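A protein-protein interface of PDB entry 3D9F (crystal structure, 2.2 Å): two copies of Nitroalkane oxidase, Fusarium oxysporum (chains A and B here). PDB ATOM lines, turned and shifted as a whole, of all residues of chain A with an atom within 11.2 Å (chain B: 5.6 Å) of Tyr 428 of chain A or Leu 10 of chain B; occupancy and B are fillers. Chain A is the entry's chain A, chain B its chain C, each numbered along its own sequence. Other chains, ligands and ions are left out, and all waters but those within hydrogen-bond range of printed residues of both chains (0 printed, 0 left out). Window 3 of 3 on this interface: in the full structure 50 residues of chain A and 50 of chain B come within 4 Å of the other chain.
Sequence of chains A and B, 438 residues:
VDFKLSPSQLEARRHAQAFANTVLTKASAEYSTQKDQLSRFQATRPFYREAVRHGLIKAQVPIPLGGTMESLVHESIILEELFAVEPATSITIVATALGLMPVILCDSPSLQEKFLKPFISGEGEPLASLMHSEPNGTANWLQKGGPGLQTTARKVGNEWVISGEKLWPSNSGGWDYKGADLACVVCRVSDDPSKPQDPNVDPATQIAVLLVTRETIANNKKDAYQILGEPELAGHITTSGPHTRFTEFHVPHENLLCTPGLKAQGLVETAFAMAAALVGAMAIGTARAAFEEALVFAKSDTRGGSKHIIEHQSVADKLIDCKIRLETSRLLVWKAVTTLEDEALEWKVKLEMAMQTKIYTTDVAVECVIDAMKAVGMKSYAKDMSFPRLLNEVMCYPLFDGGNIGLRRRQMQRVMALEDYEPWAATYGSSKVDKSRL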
ATOM      1  N   VAL A   1      23.509  29.309 -14.993  1.00  0.00           N
ATOM      2  CA  VAL A   1      22.917  29.559 -16.333  1.00  0.00           C
ATOM      3  C   VAL A   1      23.057  31.043 -16.693  1.00  0.00           C
ATOM      4  O   VAL A   1      22.907  31.930 -15.843  1.00  0.00           O
ATOM      5  CB  VAL A   1      21.430  29.069 -16.450  1.00  0.00           C
ATOM      6  CG1 VAL A   1      21.131  27.986 -15.444  1.00  0.00           C
ATOM      7  CG2 VAL A   1      20.437  30.213 -16.306  1.00  0.00           C
ATOM      8  N   LYS A 335      19.306  27.392 -27.033  1.00  0.00           N
ATOM      9  CA  LYS A 335      19.274  26.175 -26.245  1.00  0.00           C
ATOM     10  C   LYS A 335      19.674  24.986 -27.114  1.00  0.00           C
ATOM     11  O   LYS A 335      20.448  24.133 -26.684  1.00  0.00           O
ATOM     12  CB  LYS A 335      17.895  25.933 -25.619  1.00  0.00           C
ATOM     13  CG  LYS A 335      17.759  24.573 -24.919  1.00  0.00           C
ATOM     14  CD  LYS A 335      18.731  24.487 -23.726  1.00  0.00           C
ATOM     15  CE  LYS A 335      18.590  23.154 -23.006  1.00  0.00           C
ATOM     16  NZ  LYS A 335      19.290  23.289 -21.684  1.00  0.00           N
ATOM     17  N   THR A 339      22.947  22.623 -26.911  1.00  0.00           N
ATOM     18  CA  THR A 339      22.693  21.209 -26.729  1.00  0.00           C
ATOM     19  C   THR A 339      23.518  20.344 -27.694  1.00  0.00           C
ATOM     20  O   THR A 339      24.204  19.410 -27.256  1.00  0.00           O
ATOM     21  CB  THR A 339      21.185  20.913 -26.782  1.00  0.00           C
ATOM     22  OG1 THR A 339      20.557  21.619 -25.704  1.00  0.00           O
ATOM     23  CG2 THR A 339      20.898  19.443 -26.635  1.00  0.00           C
ATOM     24  N   ASP A 342      27.117  20.054 -26.635  1.00  0.00           N
ATOM     25  CA  ASP A 342      27.415  19.394 -25.371  1.00  0.00           C
ATOM     26  C   ASP A 342      27.857  17.941 -25.596  1.00  0.00           C
ATOM     27  O   ASP A 342      27.052  17.067 -25.922  1.00  0.00           O
ATOM     28  CB  ASP A 342      26.216  19.479 -24.429  1.00  0.00           C
ATOM     29  CG  ASP A 342      26.529  19.028 -23.009  1.00  0.00           C
ATOM     30  OD1 ASP A 342      27.542  18.328 -22.762  1.00  0.00           O
ATOM     31  OD2 ASP A 342      25.731  19.363 -22.111  1.00  0.00           O
ATOM     32  N   ALA A 344      28.745  15.709 -23.510  1.00  0.00           N
ATOM     33  CA  ALA A 344      28.248  14.787 -22.501  1.00  0.00           C
ATOM     34  C   ALA A 344      26.834  14.273 -22.777  1.00  0.00           C
ATOM     35  O   ALA A 344      26.308  13.475 -22.004  1.00  0.00           O
ATOM     36  CB  ALA A 344      28.314  15.434 -21.120  1.00  0.00           C
ATOM     37  N   LEU A 345      26.199  14.716 -23.861  1.00  0.00           N
ATOM     38  CA  LEU A 345      24.812  14.287 -24.104  1.00  0.00           C
ATOM     39  C   LEU A 345      24.694  13.266 -25.216  1.00  0.00           C
ATOM     40  O   LEU A 345      25.413  13.314 -26.204  1.00  0.00           O
ATOM     41  CB  LEU A 345      23.861  15.494 -24.327  1.00  0.00           C
ATOM     42  CG  LEU A 345      23.757  16.570 -23.223  1.00  0.00           C
ATOM     43  CD1 LEU A 345      22.999  17.823 -23.717  1.00  0.00           C
ATOM     44  CD2 LEU A 345      23.132  16.056 -21.911  1.00  0.00           C
ATOM     45  N   VAL A 349      19.029  12.811 -27.490  1.00  0.00           N
ATOM     46  CA  VAL A 349      18.729  14.031 -26.740  1.00  0.00           C
ATOM     47  C   VAL A 349      18.973  15.277 -27.583  1.00  0.00           C
ATOM     48  O   VAL A 349      18.179  16.230 -27.531  1.00  0.00           O
ATOM     49  CB  VAL A 349      19.570  14.140 -25.454  1.00  0.00           C
ATOM     50  CG1 VAL A 349      19.289  15.453 -24.734  1.00  0.00           C
ATOM     51  CG2 VAL A 349      19.296  12.966 -24.524  1.00  0.00           C
ATOM     52  N   GLU A 352      16.321  15.263 -30.565  1.00  0.00           N
ATOM     53  CA  GLU A 352      14.998  15.661 -30.127  1.00  0.00           C
ATOM     54  C   GLU A 352      14.925  17.167 -29.987  1.00  0.00           C
ATOM     55  O   GLU A 352      13.970  17.762 -30.440  1.00  0.00           O
ATOM     56  CB  GLU A 352      14.589  14.988 -28.808  1.00  0.00           C
ATOM     57  CG  GLU A 352      13.087  15.139 -28.509  1.00  0.00           C
ATOM     58  CD  GLU A 352      12.786  15.772 -27.139  1.00  0.00           C
ATOM     59  OE1 GLU A 352      11.652  15.635 -26.624  1.00  0.00           O
ATOM     60  OE2 GLU A 352      13.687  16.412 -26.578  1.00  0.00           O
ATOM     61  N   MET A 353      15.928  17.771 -29.354  1.00  0.00           N
ATOM     62  CA  MET A 353      15.974  19.228 -29.165  1.00  0.00           C
ATOM     63  C   MET A 353      16.022  19.954 -30.500  1.00  0.00           C
ATOM     64  O   MET A 353      15.437  21.021 -30.667  1.00  0.00           O
ATOM     65  CB  MET A 353      17.162  19.637 -28.289  1.00  0.00           C
ATOM     66  CG  MET A 353      17.212  21.126 -27.912  1.00  0.00           C
ATOM     67  SD  MET A 353      15.782  21.716 -26.954  1.00  0.00           S
ATOM     68  CE  MET A 353      16.253  21.102 -25.315  1.00  0.00           C
ATOM     69  N   GLU A 422      14.540  10.237 -22.336  1.00  0.00           N
ATOM     70  CA  GLU A 422      14.577  11.158 -21.207  1.00  0.00           C
ATOM     71  C   GLU A 422      14.201  12.568 -21.648  1.00  0.00           C
ATOM     72  O   GLU A 422      15.044  13.308 -22.175  1.00  0.00           O
ATOM     73  CB  GLU A 422      15.944  11.169 -20.542  1.00  0.00           C
ATOM     74  CG  GLU A 422      16.287   9.903 -19.802  1.00  0.00           C
ATOM     75  CD  GLU A 422      17.659  10.005 -19.164  1.00  0.00           C
ATOM     76  OE1 GLU A 422      17.703  10.324 -17.954  1.00  0.00           O
ATOM     77  OE2 GLU A 422      18.675   9.829 -19.883  1.00  0.00           O
ATOM     78  N   PRO A 423      12.931  12.935 -21.448  1.00  0.00           N
ATOM     79  CA  PRO A 423      12.422  14.219 -21.920  1.00  0.00           C
ATOM     80  C   PRO A 423      13.263  15.464 -21.538  1.00  0.00           C
ATOM     81  O   PRO A 423      13.430  16.368 -22.366  1.00  0.00           O
ATOM     82  CB  PRO A 423      10.994  14.276 -21.329  1.00  0.00           C
ATOM     83  CG  PRO A 423      10.899  13.133 -20.333  1.00  0.00           C
ATOM     84  CD  PRO A 423      11.873  12.114 -20.823  1.00  0.00           C
ATOM     85  N   TRP A 424      13.788  15.499 -20.317  1.00  0.00           N
ATOM     86  CA  TRP A 424      14.437  16.681 -19.765  1.00  0.00           C
ATOM     87  C   TRP A 424      15.946  16.526 -19.644  1.00  0.00           C
ATOM     88  O   TRP A 424      16.584  17.278 -18.901  1.00  0.00           O
ATOM     89  CB  TRP A 424      13.821  17.051 -18.402  1.00  0.00           C
ATOM     90  CG  TRP A 424      12.308  17.113 -18.481  1.00  0.00           C
ATOM     91  CD1 TRP A 424      11.410  16.356 -17.782  1.00  0.00           C
ATOM     92  CD2 TRP A 424      11.539  17.926 -19.378  1.00  0.00           C
ATOM     93  NE1 TRP A 424      10.125  16.666 -18.173  1.00  0.00           N
ATOM     94  CE2 TRP A 424      10.178  17.626 -19.151  1.00  0.00           C
ATOM     95  CE3 TRP A 424      11.871  18.888 -20.350  1.00  0.00           C
ATOM     96  CZ2 TRP A 424       9.145  18.258 -19.849  1.00  0.00           C
ATOM     97  CZ3 TRP A 424      10.839  19.520 -21.042  1.00  0.00           C
ATOM     98  CH2 TRP A 424       9.491  19.196 -20.781  1.00  0.00           C
ATOM     99  N   ALA A 425      16.529  15.587 -20.393  1.00  0.00           N
ATOM    100  CA  ALA A 425      17.961  15.309 -20.244  1.00  0.00           C
ATOM    101  C   ALA A 425      18.837  16.488 -20.652  1.00  0.00           C
ATOM    102  O   ALA A 425      19.909  16.667 -20.089  1.00  0.00           O
ATOM    103  CB  ALA A 425      18.351  14.046 -20.982  1.00  0.00           C
ATOM    104  N   ALA A 426      18.383  17.313 -21.603  1.00  0.00           N
ATOM    105  CA  ALA A 426      19.180  18.465 -22.059  1.00  0.00           C
ATOM    106  C   ALA A 426      19.079  19.612 -21.076  1.00  0.00           C
ATOM    107  O   ALA A 426      19.837  20.586 -21.147  1.00  0.00           O
ATOM    108  CB  ALA A 426      18.757  18.919 -23.441  1.00  0.00           C
ATOM    109  N   THR A 427      18.144  19.488 -20.148  1.00  0.00           N
ATOM    110  CA  THR A 427      17.954  20.506 -19.139  1.00  0.00           C
ATOM    111  C   THR A 427      18.500  20.082 -17.789  1.00  0.00           C
ATOM    112  O   THR A 427      19.253  20.817 -17.158  1.00  0.00           O
ATOM    113  CB  THR A 427      16.470  20.886 -19.032  1.00  0.00           C
ATOM    114  OG1 THR A 427      16.068  21.463 -20.277  1.00  0.00           O
ATOM    115  CG2 THR A 427      16.222  21.871 -17.891  1.00  0.00           C
ATOM    116  N   TYR A 428      18.116  18.898 -17.340  1.00  0.00           N
ATOM    117  CA  TYR A 428      18.441  18.488 -15.981  1.00  0.00           C
ATOM    118  C   TYR A 428      19.568  17.446 -15.915  1.00  0.00           C
ATOM    119  O   TYR A 428      20.003  17.052 -14.827  1.00  0.00           O
ATOM    120  CB  TYR A 428      17.159  18.057 -15.242  1.00  0.00           C
ATOM    121  CG  TYR A 428      16.219  19.216 -14.957  1.00  0.00           C
ATOM    122  CD1 TYR A 428      14.910  19.237 -15.440  1.00  0.00           C
ATOM    123  CD2 TYR A 428      16.660  20.313 -14.220  1.00  0.00           C
ATOM    124  CE1 TYR A 428      14.048  20.328 -15.161  1.00  0.00           C
ATOM    125  CE2 TYR A 428      15.825  21.392 -13.938  1.00  0.00           C
ATOM    126  CZ  TYR A 428      14.523  21.410 -14.417  1.00  0.00           C
ATOM    127  OH  TYR A 428      13.717  22.528 -14.112  1.00  0.00           O
ATOM    128  N   GLY A 429      20.089  17.057 -17.076  1.00  0.00           N
ATOM    129  CA  GLY A 429      21.081  15.986 -17.147  1.00  0.00           C
ATOM    130  C   GLY A 429      20.459  14.591 -17.188  1.00  0.00           C
ATOM    131  O   GLY A 429      19.284  14.397 -16.862  1.00  0.00           O
ATOM    132  N   SER A 430      21.252  13.610 -17.603  1.00  0.00           N
ATOM    133  CA  SER A 430      20.769  12.232 -17.716  1.00  0.00           C
ATOM    134  C   SER A 430      20.795  11.469 -16.382  1.00  0.00           C
ATOM    135  O   SER A 430      21.443  11.898 -15.437  1.00  0.00           O
ATOM    136  CB  SER A 430      21.590  11.490 -18.763  1.00  0.00           C
ATOM    137  OG  SER A 430      20.988  10.243 -19.040  1.00  0.00           O
ATOM    138  N   SER A 431      20.094  10.335 -16.316  1.00  0.00           N
ATOM    139  CA  SER A 431      20.123   9.458 -15.133  1.00  0.00           C
ATOM    140  C   SER A 431      20.574   8.023 -15.450  1.00  0.00           C
ATOM    141  O   SER A 431      21.505   7.796 -16.240  1.00  0.00           O
ATOM    142  CB  SER A 431      18.767   9.450 -14.446  1.00  0.00           C
ATOM    143  N   LEU B   5      23.421  23.668 -15.252  1.00  0.00           N
ATOM    144  CA  LEU B   5      23.041  23.872 -13.867  1.00  0.00           C
ATOM    145  C   LEU B   5      24.227  23.580 -12.966  1.00  0.00           C
ATOM    146  O   LEU B   5      24.932  22.595 -13.161  1.00  0.00           O
ATOM    147  CB  LEU B   5      21.842  22.997 -13.495  1.00  0.00           C
ATOM    148  CG  LEU B   5      20.534  23.287 -14.254  1.00  0.00           C
ATOM    149  CD1 LEU B   5      19.439  22.318 -13.860  1.00  0.00           C
ATOM    150  CD2 LEU B   5      20.064  24.717 -14.046  1.00  0.00           C
ATOM    151  N   SER B   6      24.446  24.458 -11.992  1.00  0.00           N
ATOM    152  CA  SER B   6      25.475  24.273 -10.976  1.00  0.00           C
ATOM    153  C   SER B   6      25.078  23.168  -9.981  1.00  0.00           C
ATOM    154  O   SER B   6      23.901  22.834  -9.855  1.00  0.00           O
ATOM    155  CB  SER B   6      25.674  25.585 -10.228  1.00  0.00           C
ATOM    156  OG  SER B   6      24.524  25.898  -9.449  1.00  0.00           O
ATOM    157  N   PRO B   7      26.063  22.600  -9.254  1.00  0.00           N
ATOM    158  CA  PRO B   7      25.713  21.648  -8.201  1.00  0.00           C
ATOM    159  C   PRO B   7      24.608  22.129  -7.242  1.00  0.00           C
ATOM    160  O   PRO B   7      23.782  21.321  -6.809  1.00  0.00           O
ATOM    161  CB  PRO B   7      27.036  21.475  -7.441  1.00  0.00           C
ATOM    162  CG  PRO B   7      28.108  21.743  -8.472  1.00  0.00           C
ATOM    163  CD  PRO B   7      27.526  22.785  -9.387  1.00  0.00           C
ATOM    164  N   SER B   8      24.583  23.416  -6.900  1.00  0.00           N
ATOM    165  CA  SER B   8      23.603  23.881  -5.908  1.00  0.00           C
ATOM    166  C   SER B   8      22.177  24.021  -6.485  1.00  0.00           C
ATOM    167  O   SER B   8      21.187  23.969  -5.748  1.00  0.00           O
ATOM    168  CB  SER B   8      24.076  25.158  -5.218  1.00  0.00           C
ATOM    169  OG  SER B   8      23.922  26.281  -6.049  1.00  0.00           O
ATOM    170  N   GLN B   9      22.092  24.175  -7.802  1.00  0.00           N
ATOM    171  CA  GLN B   9      20.820  24.197  -8.514  1.00  0.00           C
ATOM    172  C   GLN B   9      20.270  22.785  -8.673  1.00  0.00           C
ATOM    173  O   GLN B   9      19.074  22.542  -8.456  1.00  0.00           O
ATOM    174  CB  GLN B   9      20.989  24.867  -9.867  1.00  0.00           C
ATOM    175  CG  GLN B   9      21.053  26.358  -9.732  1.00  0.00           C
ATOM    176  CD  GLN B   9      21.615  27.068 -10.949  1.00  0.00           C
ATOM    177  OE1 GLN B   9      22.385  26.504 -11.727  1.00  0.00           O
ATOM    178  NE2 GLN B   9      21.231  28.327 -11.108  1.00  0.00           N
ATOM    179  N   LEU B  10      21.150  21.851  -9.032  1.00  0.00           N
ATOM    180  CA  LEU B  10      20.794  20.431  -9.035  1.00  0.00           C
ATOM    181  C   LEU B  10      20.357  19.950  -7.645  1.00  0.00           C
ATOM    182  O   LEU B  10      19.386  19.200  -7.516  1.00  0.00           O
ATOM    183  CB  LEU B  10      21.946  19.595  -9.589  1.00  0.00           C
ATOM    184  CG  LEU B  10      22.202  19.846 -11.088  1.00  0.00           C
ATOM    185  CD1 LEU B  10      23.527  19.270 -11.521  1.00  0.00           C
ATOM    186  CD2 LEU B  10      21.058  19.282 -11.940  1.00  0.00           C
ATOM    187  N   GLU B  11      21.056  20.412  -6.612  1.00  0.00           N
ATOM    188  CA  GLU B  11      20.712  20.065  -5.234  1.00  0.00           C
ATOM    189  C   GLU B  11      19.388  20.693  -4.801  1.00  0.00           C
ATOM    190  O   GLU B  11      18.617  20.050  -4.081  1.00  0.00           O
ATOM    191  CB  GLU B  11      21.847  20.405  -4.252  1.00  0.00           C
ATOM    192  CG  GLU B  11      21.441  20.336  -2.749  1.00  0.00           C
ATOM    193  CD  GLU B  11      20.947  18.952  -2.281  1.00  0.00           C
ATOM    194  OE1 GLU B  11      20.117  18.897  -1.342  1.00  0.00           O
ATOM    195  OE2 GLU B  11      21.385  17.918  -2.845  1.00  0.00           O
ATOM    196  N   ALA B  12      19.124  21.931  -5.230  1.00  0.00           N
ATOM    197  CA  ALA B  12      17.822  22.568  -4.966  1.00  0.00           C
ATOM    198  C   ALA B  12      16.670  21.812  -5.629  1.00  0.00           C
ATOM    199  O   ALA B  12      15.591  21.697  -5.060  1.00  0.00           O
ATOM    200  CB  ALA B  12      17.815  24.014  -5.398  1.00  0.00           C
ATOM    201  N   ARG B  13      16.907  21.317  -6.837  1.00  0.00           N
ATOM    202  CA  ARG B  13      15.945  20.460  -7.520  1.00  0.00           C
ATOM    203  C   ARG B  13      15.697  19.170  -6.706  1.00  0.00           C
ATOM    204  O   ARG B  13      14.562  18.869  -6.334  1.00  0.00           O
ATOM    205  CB  ARG B  13      16.460  20.123  -8.928  1.00  0.00           C
ATOM    206  CG  ARG B  13      15.453  19.369  -9.755  1.00  0.00           C
ATOM    207  CD  ARG B  13      15.977  19.019 -11.120  1.00  0.00           C
ATOM    208  NE  ARG B  13      14.862  18.483 -11.881  1.00  0.00           N
ATOM    209  CZ  ARG B  13      14.781  17.239 -12.335  1.00  0.00           C
ATOM    210  NH1 ARG B  13      15.804  16.398 -12.167  1.00  0.00           N
ATOM    211  NH2 ARG B  13      13.676  16.861 -12.989  1.00  0.00           N
ATOM    212  N   ARG B  14      16.780  18.445  -6.414  1.00  0.00           N
ATOM    213  CA  ARG B  14      16.725  17.204  -5.625  1.00  0.00           C
ATOM    214  C   ARG B  14      15.936  17.397  -4.333  1.00  0.00           C
ATOM    215  O   ARG B  14      15.051  16.590  -4.016  1.00  0.00           O
ATOM    216  CB  ARG B  14      18.143  16.710  -5.288  1.00  0.00           C
ATOM    217  CG  ARG B  14      18.170  15.320  -4.597  1.00  0.00           C
ATOM    218  CD  ARG B  14      19.363  15.160  -3.649  1.00  0.00           C
ATOM    219  NE  ARG B  14      19.297  16.093  -2.525  1.00  0.00           N
ATOM    220  CZ  ARG B  14      18.487  15.971  -1.473  1.00  0.00           C
ATOM    221  NH1 ARG B  14      17.649  14.942  -1.373  1.00  0.00           N
ATOM    222  NH2 ARG B  14      18.507  16.890  -0.516  1.00  0.00           N
ATOM    223  N   HIS B  15      16.267  18.467  -3.602  1.00  0.00           N
ATOM    224  CA  HIS B  15      15.589  18.834  -2.354  1.00  0.00           C
ATOM    225  C   HIS B  15      14.100  19.168  -2.526  1.00  0.00           C
ATOM    226  O   HIS B  15      13.270  18.748  -1.724  1.00  0.00           O
ATOM    227  CB  HIS B  15      16.318  20.005  -1.697  1.00  0.00           C
ATOM    228  CG  HIS B  15      15.648  20.527  -0.470  1.00  0.00           C
ATOM    229  ND1 HIS B  15      16.055  20.180   0.804  1.00  0.00           N
ATOM    230  CD2 HIS B  15      14.620  21.393  -0.315  1.00  0.00           C
ATOM    231  CE1 HIS B  15      15.293  20.798   1.690  1.00  0.00           C
ATOM    232  NE2 HIS B  15      14.414  21.540   1.039  1.00  0.00           N
ATOM    233  N   ILE B  77      13.423  26.582 -10.274  1.00  0.00           N
ATOM    234  CA  ILE B  77      13.610  25.125 -10.273  1.00  0.00           C
ATOM    235  C   ILE B  77      12.731  24.503  -9.188  1.00  0.00           C
ATOM    236  O   ILE B  77      11.986  23.533  -9.435  1.00  0.00           O
ATOM    237  CB  ILE B  77      15.122  24.748 -10.124  1.00  0.00           C
ATOM    238  CG1 ILE B  77      15.859  24.967 -11.447  1.00  0.00           C
ATOM    239  CG2 ILE B  77      15.319  23.292  -9.698  1.00  0.00           C
ATOM    240  CD1 ILE B  77      17.402  24.998 -11.313  1.00  0.00           C
ATOM    241  N   GLU B  80       8.841  24.727  -9.977  1.00  0.00           N
ATOM    242  CA  GLU B  80       8.464  23.768 -10.990  1.00  0.00           C
ATOM    243  C   GLU B  80       8.259  22.391 -10.391  1.00  0.00           C
ATOM    244  O   GLU B  80       7.208  21.784 -10.589  1.00  0.00           O
ATOM    245  CB  GLU B  80       9.479  23.706 -12.134  1.00  0.00           C
ATOM    246  CG  GLU B  80       9.103  22.660 -13.193  1.00  0.00           C
ATOM    247  CD  GLU B  80      10.096  22.575 -14.337  1.00  0.00           C
ATOM    248  OE1 GLU B  80      10.035  21.582 -15.101  1.00  0.00           O
ATOM    249  OE2 GLU B  80      10.913  23.516 -14.503  1.00  0.00           O
ATOM    250  N   GLU B  81       9.255  21.927  -9.635  1.00  0.00           N
ATOM    251  CA  GLU B  81       9.224  20.612  -8.968  1.00  0.00           C
ATOM    252  C   GLU B  81       8.090  20.473  -7.943  1.00  0.00           C
ATOM    253  O   GLU B  81       7.466  19.417  -7.820  1.00  0.00           O
ATOM    254  CB  GLU B  81      10.577  20.325  -8.284  1.00  0.00           C
ATOM    255  CG  GLU B  81      11.742  20.083  -9.244  1.00  0.00           C
ATOM    256  CD  GLU B  81      11.422  19.075 -10.344  1.00  0.00           C
ATOM    257  OE1 GLU B  81      10.689  18.077 -10.091  1.00  0.00           O
ATOM    258  OE2 GLU B  81      11.921  19.268 -11.470  1.00  0.00           O
ATOM    259  N   ARG B 288       3.620  20.241 -16.937  1.00  0.00           N
ATOM    260  CA  ARG B 288       4.565  19.119 -16.954  1.00  0.00           C
ATOM    261  C   ARG B 288       3.989  17.816 -16.366  1.00  0.00           C
ATOM    262  O   ARG B 288       4.225  16.722 -16.894  1.00  0.00           O
ATOM    263  CB  ARG B 288       5.872  19.484 -16.221  1.00  0.00           C
ATOM    264  CG  ARG B 288       6.972  18.446 -16.448  1.00  0.00           C
ATOM    265  CD  ARG B 288       8.248  18.796 -15.707  1.00  0.00           C
ATOM    266  NE  ARG B 288       8.300  18.172 -14.389  1.00  0.00           N
ATOM    267  CZ  ARG B 288       9.223  18.429 -13.459  1.00  0.00           C
ATOM    268  NH1 ARG B 288      10.190  19.325 -13.676  1.00  0.00           N
ATOM    269  NH2 ARG B 288       9.176  17.795 -12.286  1.00  0.00           N
ATOM    270  N   ARG B 330      10.006  27.140 -20.143  1.00  0.00           N
ATOM    271  CA  ARG B 330      11.040  27.110 -19.111  1.00  0.00           C
ATOM    272  C   ARG B 330      12.194  28.032 -19.495  1.00  0.00           C
ATOM    273  O   ARG B 330      12.726  28.745 -18.656  1.00  0.00           O
ATOM    274  CB  ARG B 330      11.518  25.675 -18.858  1.00  0.00           C
ATOM    275  CG  ARG B 330      12.431  25.566 -17.659  1.00  0.00           C
ATOM    276  CD  ARG B 330      13.082  24.191 -17.545  1.00  0.00           C
ATOM    277  NE  ARG B 330      12.073  23.181 -17.254  1.00  0.00           N
ATOM    278  CZ  ARG B 330      11.678  22.258 -18.120  1.00  0.00           C
ATOM    279  NH1 ARG B 330      12.193  22.228 -19.338  1.00  0.00           N
ATOM    280  NH2 ARG B 330      10.757  21.367 -17.766  1.00  0.00           N
ATOM    281  N   TRP B 334      13.572  31.227 -17.303  1.00  0.00           N
ATOM    282  CA  TRP B 334      14.969  31.414 -16.871  1.00  0.00           C
ATOM    283  C   TRP B 334      15.527  32.685 -17.495  1.00  0.00           C
ATOM    284  O   TRP B 334      16.249  33.413 -16.832  1.00  0.00           O
ATOM    285  CB  TRP B 334      15.847  30.193 -17.177  1.00  0.00           C
ATOM    286  CG  TRP B 334      15.471  28.948 -16.397  1.00  0.00           C
ATOM    287  CD1 TRP B 334      14.394  28.779 -15.578  1.00  0.00           C
ATOM    288  CD2 TRP B 334      16.163  27.689 -16.411  1.00  0.00           C
ATOM    289  NE1 TRP B 334      14.375  27.499 -15.071  1.00  0.00           N
ATOM    290  CE2 TRP B 334      15.452  26.810 -15.566  1.00  0.00           C
ATOM    291  CE3 TRP B 334      17.322  27.221 -17.062  1.00  0.00           C
ATOM    292  CZ2 TRP B 334      15.856  25.491 -15.345  1.00  0.00           C
ATOM    293  CZ3 TRP B 334      17.728  25.901 -16.844  1.00  0.00           C
ATOM    294  CH2 TRP B 334      16.991  25.053 -15.995  1.00  0.00           C
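The side-chain hydroxyl (OH) of Tyr 428 of chain A sits at hydrogen-bond distance from the side-chain carboxylate (OE2) of Glu 80 of chain B (3.0 Å).
The side-chain carboxylate (OE1) of Glu 80 of chain B is in salt-bridge range of the guanidinium group (NH2) of Arg 330 of chain B (2.8 Å).
OE2 of Glu 81 of chain B is in salt-bridge range of NE of Arg 13 of chain B, at 3.1 Å.
The side-chain carboxylate (OE1) of Glu 81 of chain B lies within salt-bridge range of the guanidinium group (NH2) of Arg 288 of chain B (2.7 Å).
The side-chain carboxylate (OE1) of Glu 80 of chain B is in salt-bridge range of the guanidinium group (NH1) of Arg 288 of chain B.
Among the printed residues, merely in contact across the chains: Val 1 of chain A with Leu 5 of chain B (3.7 Å), Trp 424 of chain A with Arg 288 of chain B (3.8 Å), Trp 424 of chain A with Arg 330 of chain B (3.5 Å), Thr 427 of chain A with Leu 5 of chain B (3.6 Å), Thr 427 of chain A with Arg 330 of chain B (3.9 Å), Thr 427 of chain A with Trp 334 of chain B (3.8 Å), Tyr 428 of chain A with Leu 5 of chain B (3.4 Å), Tyr 428 of chain A with Leu 10 of chain B (3.8 Å), Tyr 428 of chain A with Arg 13 of chain B (3.4 Å), Tyr 428 of chain A with Arg 330 of chain B (3.6 Å) and Tyr 428 of chain A with Trp 334 of chain B (3.9 Å).
Of the printed residues of chain B, Tyr 428 of chain A touches Leu 5, Leu 10, Arg 13, Glu 80, Arg 330 and Trp 334.
Leu 10 of chain B touches just one residue of chain A: Tyr 428 (3.8 Å).
Leu 5 of chain B touches three residues of chain A.
No residue of chain A comes within 4 Å of Pro 7 of chain B.
No residue of chain A comes within 4 Å of Ser 8 of chain B.
No residue of chain A comes within 4 Å of Ala 12 of chain B.
Of chain A, only Tyr 428 (3.4 Å) comes within 4 Å of Arg 13 of chain B.
No residue of chain A comes within 4 Å of Ile 77 of chain B.
Printed residues of chain A within 4 Å of Glu 80 of chain B: Tyr 428.
Of the printed residues of chain A, Trp 334 of chain B touches Thr 427 (3.8 Å) and Tyr 428 (3.9 Å).
Of the printed residues of chain A, Arg 288 of chain B touches Trp 424.
Glu 422 of chain A touches none of the printed residues of chain B.
Ala 426 of chain A touches none of the printed residues of chain B.
The nearest residue of chain B that does not touch Tyr 428 of chain A is Ile 77 of chain B (4.2 Å).
Printed residues of chain B that touch a printed residue of chain A: Leu 5, Leu 10, Arg 13, Glu 80, Arg 288, Arg 330 and Trp 334.
Hydrophobic or aromatic side chains of chain B that line the printed part of chain A: Leu 5, Leu 10 and Trp 334.
Along chain A the printed residues that touch a printed residue of chain B span positions 1 to 428.
Among the printed residues, 12 pairs touch across the chains.
No position is printed for both chains.
Of the 12 pairs that touch across the chains among the printed residues, none has its exchanged pair printed and touching as well.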
